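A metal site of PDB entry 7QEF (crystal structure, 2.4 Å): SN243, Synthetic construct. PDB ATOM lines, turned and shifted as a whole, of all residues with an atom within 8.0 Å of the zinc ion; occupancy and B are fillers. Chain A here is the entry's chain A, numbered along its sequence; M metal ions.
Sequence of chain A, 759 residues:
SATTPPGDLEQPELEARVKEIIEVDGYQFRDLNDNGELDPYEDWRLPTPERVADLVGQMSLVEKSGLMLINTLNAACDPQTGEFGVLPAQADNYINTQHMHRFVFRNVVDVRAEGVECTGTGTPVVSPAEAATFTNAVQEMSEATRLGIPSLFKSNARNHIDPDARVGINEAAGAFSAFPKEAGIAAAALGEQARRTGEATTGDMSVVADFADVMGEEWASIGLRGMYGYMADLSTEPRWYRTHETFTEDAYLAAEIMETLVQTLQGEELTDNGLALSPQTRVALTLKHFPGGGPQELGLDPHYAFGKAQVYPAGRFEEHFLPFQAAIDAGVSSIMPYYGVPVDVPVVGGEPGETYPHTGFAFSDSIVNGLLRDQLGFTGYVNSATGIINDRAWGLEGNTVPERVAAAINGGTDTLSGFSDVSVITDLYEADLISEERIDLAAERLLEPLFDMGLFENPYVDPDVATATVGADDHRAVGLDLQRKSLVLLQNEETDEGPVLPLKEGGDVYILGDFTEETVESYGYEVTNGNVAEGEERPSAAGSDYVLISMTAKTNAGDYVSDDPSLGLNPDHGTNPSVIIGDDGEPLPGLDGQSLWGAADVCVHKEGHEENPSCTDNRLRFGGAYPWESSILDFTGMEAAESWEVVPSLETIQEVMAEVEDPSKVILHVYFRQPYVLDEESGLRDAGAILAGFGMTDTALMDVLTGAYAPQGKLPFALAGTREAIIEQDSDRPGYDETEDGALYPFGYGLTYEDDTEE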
ATOM      1  N   GLU A  20     -12.157 -23.129 -24.941  1.00  0.00           N
ATOM      2  CA  GLU A  20     -12.949 -24.338 -25.298  1.00  0.00           C
ATOM      3  C   GLU A  20     -12.344 -25.602 -24.695  1.00  0.00           C
ATOM      4  O   GLU A  20     -11.238 -25.535 -24.139  1.00  0.00           O
ATOM      5  CB  GLU A  20     -13.077 -24.460 -26.819  1.00  0.00           C
ATOM      6  CG  GLU A  20     -14.218 -23.642 -27.380  1.00  0.00           C
ATOM      7  CD  GLU A  20     -15.574 -23.963 -26.762  1.00  0.00           C
ATOM      8  OE1 GLU A  20     -15.739 -25.098 -26.264  1.00  0.00           O
ATOM      9  OE2 GLU A  20     -16.455 -23.089 -26.765  1.00  0.00           O
ATOM     10  N   ILE A  22     -10.874 -29.532 -24.958  1.00  0.00           N
ATOM     11  CA  ILE A  22     -10.144 -30.385 -25.939  1.00  0.00           C
ATOM     12  C   ILE A  22     -10.144 -31.825 -25.417  1.00  0.00           C
ATOM     13  O   ILE A  22      -9.881 -32.016 -24.210  1.00  0.00           O
ATOM     14  CB  ILE A  22      -8.718 -29.845 -26.156  1.00  0.00           C
ATOM     15  CG1 ILE A  22      -7.862 -29.979 -24.891  1.00  0.00           C
ATOM     16  CG2 ILE A  22      -8.759 -28.416 -26.661  1.00  0.00           C
ATOM     17  CD1 ILE A  22      -6.459 -29.460 -25.054  1.00  0.00           C
ATOM     18  N   ARG A  30      -9.570 -28.479 -20.499  1.00  0.00           N
ATOM     19  CA  ARG A  30      -9.826 -27.065 -20.891  1.00  0.00           C
ATOM     20  C   ARG A  30      -8.560 -26.484 -21.520  1.00  0.00           C
ATOM     21  O   ARG A  30      -7.514 -26.479 -20.839  1.00  0.00           O
ATOM     22  CB  ARG A  30     -10.259 -26.238 -19.680  1.00  0.00           C
ATOM     23  CG  ARG A  30     -11.577 -26.676 -19.059  1.00  0.00           C
ATOM     24  CD  ARG A  30     -12.293 -25.495 -18.430  1.00  0.00           C
ATOM     25  NE  ARG A  30     -11.500 -24.831 -17.403  1.00  0.00           N
ATOM     26  CZ  ARG A  30     -11.745 -23.620 -16.940  1.00  0.00           C
ATOM     27  NH1 ARG A  30     -10.969 -23.096 -16.009  1.00  0.00           N
ATOM     28  NH2 ARG A  30     -12.759 -22.914 -17.421  1.00  0.00           N
ATOM     29  N   ASP A  31      -8.660 -26.001 -22.753  1.00  0.00           N
ATOM     30  CA  ASP A  31      -7.503 -25.363 -23.404  1.00  0.00           C
ATOM     31  C   ASP A  31      -7.489 -23.891 -23.037  1.00  0.00           C
ATOM     32  O   ASP A  31      -8.064 -23.046 -23.723  1.00  0.00           O
ATOM     33  CB  ASP A  31      -7.538 -25.545 -24.919  1.00  0.00           C
ATOM     34  CG  ASP A  31      -6.205 -25.181 -25.569  1.00  0.00           C
ATOM     35  OD1 ASP A  31      -5.190 -25.204 -24.858  1.00  0.00           O
ATOM     36  OD2 ASP A  31      -6.177 -24.857 -26.770  1.00  0.00           O
ATOM     37  N   LEU A  32      -6.752 -23.583 -21.976  1.00  0.00           N
ATOM     38  CA  LEU A  32      -6.811 -22.257 -21.382  1.00  0.00           C
ATOM     39  C   LEU A  32      -5.857 -21.266 -22.018  1.00  0.00           C
ATOM     40  O   LEU A  32      -6.163 -20.057 -22.030  1.00  0.00           O
ATOM     41  CB  LEU A  32      -6.552 -22.362 -19.872  1.00  0.00           C
ATOM     42  CG  LEU A  32      -7.677 -23.133 -19.164  1.00  0.00           C
ATOM     43  CD1 LEU A  32      -7.266 -23.625 -17.776  1.00  0.00           C
ATOM     44  CD2 LEU A  32      -8.974 -22.305 -19.071  1.00  0.00           C
ATOM     45  N   ASN A  33      -4.713 -21.734 -22.557  1.00  0.00           N
ATOM     46  CA  ASN A  33      -3.845 -20.873 -23.363  1.00  0.00           C
ATOM     47  C   ASN A  33      -4.379 -20.690 -24.767  1.00  0.00           C
ATOM     48  O   ASN A  33      -3.844 -19.845 -25.496  1.00  0.00           O
ATOM     49  CB  ASN A  33      -2.412 -21.395 -23.455  1.00  0.00           C
ATOM     50  CG  ASN A  33      -2.342 -22.853 -23.793  1.00  0.00           C
ATOM     51  OD1 ASN A  33      -3.203 -23.372 -24.508  1.00  0.00           O
ATOM     52  ND2 ASN A  33      -1.284 -23.517 -23.334  1.00  0.00           N
ATOM     53  N   ASP A  34      -5.387 -21.469 -25.179  1.00  0.00           N
ATOM     54  CA  ASP A  34      -6.001 -21.347 -26.495  1.00  0.00           C
ATOM     55  C   ASP A  34      -4.958 -21.520 -27.591  1.00  0.00           C
ATOM     56  O   ASP A  34      -4.935 -20.801 -28.589  1.00  0.00           O
ATOM     57  CB  ASP A  34      -6.761 -20.011 -26.600  1.00  0.00           C
ATOM     58  CG  ASP A  34      -7.458 -19.799 -27.932  1.00  0.00           C
ATOM     59  OD1 ASP A  34      -8.496 -20.447 -28.238  1.00  0.00           O
ATOM     60  OD2 ASP A  34      -6.946 -18.934 -28.675  1.00  0.00           O
ATOM     61  N   ASN A  35      -4.093 -22.524 -27.376  1.00  0.00           N
ATOM     62  CA  ASN A  35      -3.032 -22.866 -28.347  1.00  0.00           C
ATOM     63  C   ASN A  35      -3.508 -24.052 -29.181  1.00  0.00           C
ATOM     64  O   ASN A  35      -2.906 -24.331 -30.224  1.00  0.00           O
ATOM     65  CB  ASN A  35      -1.739 -23.265 -27.642  1.00  0.00           C
ATOM     66  CG  ASN A  35      -1.892 -24.496 -26.776  1.00  0.00           C
ATOM     67  OD1 ASN A  35      -2.994 -25.020 -26.615  1.00  0.00           O
ATOM     68  ND2 ASN A  35      -0.793 -24.966 -26.205  1.00  0.00           N
ATOM     69  N   GLY A  36      -4.557 -24.739 -28.715  1.00  0.00           N
ATOM     70  CA  GLY A  36      -5.120 -25.882 -29.442  1.00  0.00           C
ATOM     71  C   GLY A  36      -4.507 -27.182 -28.971  1.00  0.00           C
ATOM     72  O   GLY A  36      -4.840 -28.236 -29.544  1.00  0.00           O
ATOM     73  N   GLU A  37      -3.635 -27.116 -27.973  1.00  0.00           N
ATOM     74  CA  GLU A  37      -2.934 -28.345 -27.524  1.00  0.00           C
ATOM     75  C   GLU A  37      -3.023 -28.453 -26.002  1.00  0.00           C
ATOM     76  O   GLU A  37      -3.218 -27.423 -25.336  1.00  0.00           O
ATOM     77  CB  GLU A  37      -1.480 -28.325 -28.000  1.00  0.00           C
ATOM     78  CG  GLU A  37      -0.869 -29.707 -28.089  1.00  0.00           C
ATOM     79  CD  GLU A  37       0.399 -29.794 -28.917  1.00  0.00           C
ATOM     80  OE1 GLU A  37       0.999 -28.738 -29.176  1.00  0.00           O
ATOM     81  OE2 GLU A  37       0.772 -30.916 -29.304  1.00  0.00           O
ATOM     82  N   LEU A  38      -2.892 -29.680 -25.481  1.00  0.00           N
ATOM     83  CA  LEU A  38      -2.987 -29.883 -24.020  1.00  0.00           C
ATOM     84  C   LEU A  38      -1.640 -29.551 -23.389  1.00  0.00           C
ATOM     85  O   LEU A  38      -0.652 -30.222 -23.719  1.00  0.00           O
ATOM     86  CB  LEU A  38      -3.357 -31.347 -23.738  1.00  0.00           C
ATOM     87  CG  LEU A  38      -3.355 -31.740 -22.258  1.00  0.00           C
ATOM     88  CD1 LEU A  38      -4.332 -30.893 -21.464  1.00  0.00           C
ATOM     89  CD2 LEU A  38      -3.673 -33.215 -22.095  1.00  0.00           C
ATOM     90  N   ASP A  39      -1.614 -28.554 -22.500  1.00  0.00           N
ATOM     91  CA  ASP A  39      -0.360 -28.250 -21.771  1.00  0.00           C
ATOM     92  C   ASP A  39      -0.428 -28.961 -20.425  1.00  0.00           C
ATOM     93  O   ASP A  39      -1.543 -29.130 -19.902  1.00  0.00           O
ATOM     94  CB  ASP A  39      -0.126 -26.741 -21.692  1.00  0.00           C
ATOM     95  CG  ASP A  39      -0.219 -26.046 -23.029  1.00  0.00           C
ATOM     96  OD1 ASP A  39      -1.263 -26.189 -23.697  1.00  0.00           O
ATOM     97  OD2 ASP A  39       0.751 -25.369 -23.401  1.00  0.00           O
ATOM     98  N   PRO A  40       0.711 -29.421 -19.857  1.00  0.00           N
ATOM     99  CA  PRO A  40       0.675 -30.181 -18.615  1.00  0.00           C
ATOM    100  C   PRO A  40      -0.127 -29.482 -17.506  1.00  0.00           C
ATOM    101  O   PRO A  40      -0.670 -30.171 -16.666  1.00  0.00           O
ATOM    102  CB  PRO A  40       2.164 -30.257 -18.230  1.00  0.00           C
ATOM    103  CG  PRO A  40       2.884 -30.196 -19.561  1.00  0.00           C
ATOM    104  CD  PRO A  40       2.052 -29.264 -20.403  1.00  0.00           C
ATOM    105  N   TYR A  41      -0.181 -28.149 -17.510  1.00  0.00           N
ATOM    106  CA  TYR A  41      -0.902 -27.404 -16.455  1.00  0.00           C
ATOM    107  C   TYR A  41      -2.415 -27.542 -16.681  1.00  0.00           C
ATOM    108  O   TYR A  41      -3.161 -27.496 -15.689  1.00  0.00           O
ATOM    109  CB  TYR A  41      -0.431 -25.943 -16.395  1.00  0.00           C
ATOM    110  CG  TYR A  41      -1.178 -24.950 -17.246  1.00  0.00           C
ATOM    111  CD1 TYR A  41      -2.351 -24.365 -16.802  1.00  0.00           C
ATOM    112  CD2 TYR A  41      -0.689 -24.547 -18.487  1.00  0.00           C
ATOM    113  CE1 TYR A  41      -3.031 -23.435 -17.571  1.00  0.00           C
ATOM    114  CE2 TYR A  41      -1.362 -23.619 -19.263  1.00  0.00           C
ATOM    115  CZ  TYR A  41      -2.535 -23.058 -18.800  1.00  0.00           C
ATOM    116  OH  TYR A  41      -3.204 -22.142 -19.569  1.00  0.00           O
ATOM    117  N   GLU A  42      -2.826 -27.721 -17.934  1.00  0.00           N
ATOM    118  CA  GLU A  42      -4.264 -27.909 -18.262  1.00  0.00           C
ATOM    119  C   GLU A  42      -4.641 -29.380 -18.074  1.00  0.00           C
ATOM    120  O   GLU A  42      -5.829 -29.702 -18.201  1.00  0.00           O
ATOM    121  CB  GLU A  42      -4.511 -27.440 -19.692  1.00  0.00           C
ATOM    122  CG  GLU A  42      -4.079 -26.016 -19.960  1.00  0.00           C
ATOM    123  CD  GLU A  42      -4.063 -25.610 -21.424  1.00  0.00           C
ATOM    124  OE1 GLU A  42      -3.939 -26.499 -22.277  1.00  0.00           O
ATOM    125  OE2 GLU A  42      -4.171 -24.404 -21.695  1.00  0.00           O
ATOM    126  N   ASP A  54       4.588 -26.061 -15.042  1.00  0.00           N
ATOM    127  CA  ASP A  54       4.313 -25.755 -16.443  1.00  0.00           C
ATOM    128  C   ASP A  54       3.616 -24.409 -16.600  1.00  0.00           C
ATOM    129  O   ASP A  54       3.865 -23.678 -17.568  1.00  0.00           O
ATOM    130  CB  ASP A  54       3.472 -26.857 -17.090  1.00  0.00           C
ATOM    131  CG  ASP A  54       3.313 -26.668 -18.583  1.00  0.00           C
ATOM    132  OD1 ASP A  54       4.311 -26.878 -19.308  1.00  0.00           O
ATOM    133  OD2 ASP A  54       2.206 -26.287 -19.029  1.00  0.00           O
ATOM    134  N   GLN A  58       5.384 -20.729 -18.280  1.00  0.00           N
ATOM    135  CA  GLN A  58       4.849 -19.964 -19.394  1.00  0.00           C
ATOM    136  C   GLN A  58       4.473 -18.539 -19.064  1.00  0.00           C
ATOM    137  O   GLN A  58       3.981 -17.829 -19.946  1.00  0.00           O
ATOM    138  CB  GLN A  58       3.581 -20.636 -19.939  1.00  0.00           C
ATOM    139  CG  GLN A  58       3.704 -22.073 -20.328  1.00  0.00           C
ATOM    140  CD  GLN A  58       2.374 -22.666 -20.704  1.00  0.00           C
ATOM    141  OE1 GLN A  58       1.521 -21.974 -21.276  1.00  0.00           O
ATOM    142  NE2 GLN A  58       2.181 -23.934 -20.402  1.00  0.00           N
HETATM  143 ZN    ZN M   1      -3.349 -25.466 -24.272  1.00  0.00          ZN
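Within 4 Å of the zinc ion: Asp 31, Asn 33, Asn 35, Glu 37, Asp 39 and Glu 42. Along chain A the residues within 4 Å of the zinc ion span positions 31 to 42. The nearest printed residue that does not touch the zinc ion is Leu 38 (4.4 Å).
The zinc ion is bound by the side-chain carboxylate of Asp 31, the side-chain amide oxygen of Asn 33, the backbone carbonyl oxygen of Glu 37, the side-chain carboxylate of Asp 39, the side-chain carboxylate of Glu 42 and the side-chain amide oxygen of Asn 35.
N of Gly 36 lies within hydrogen-bond range of OD2 of Asp 31 (2.5 Å). O of Glu 20 lies within hydrogen-bond range of N of Asp 31, 3.0 Å away. The backbone NH (N) of Asn 33 lies within hydrogen-bond range of the side-chain hydroxyl (OH) of Tyr 41 (3.4 Å). The backbone NH (N) of Leu 32 is in hydrogen-bond range of the side-chain carboxylate (OE2) of Glu 42. The side-chain hydroxyl (OH) of Tyr 41 is in hydrogen-bond range of the side-chain carboxylate (OE2) of Glu 42 (3.3 Å).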
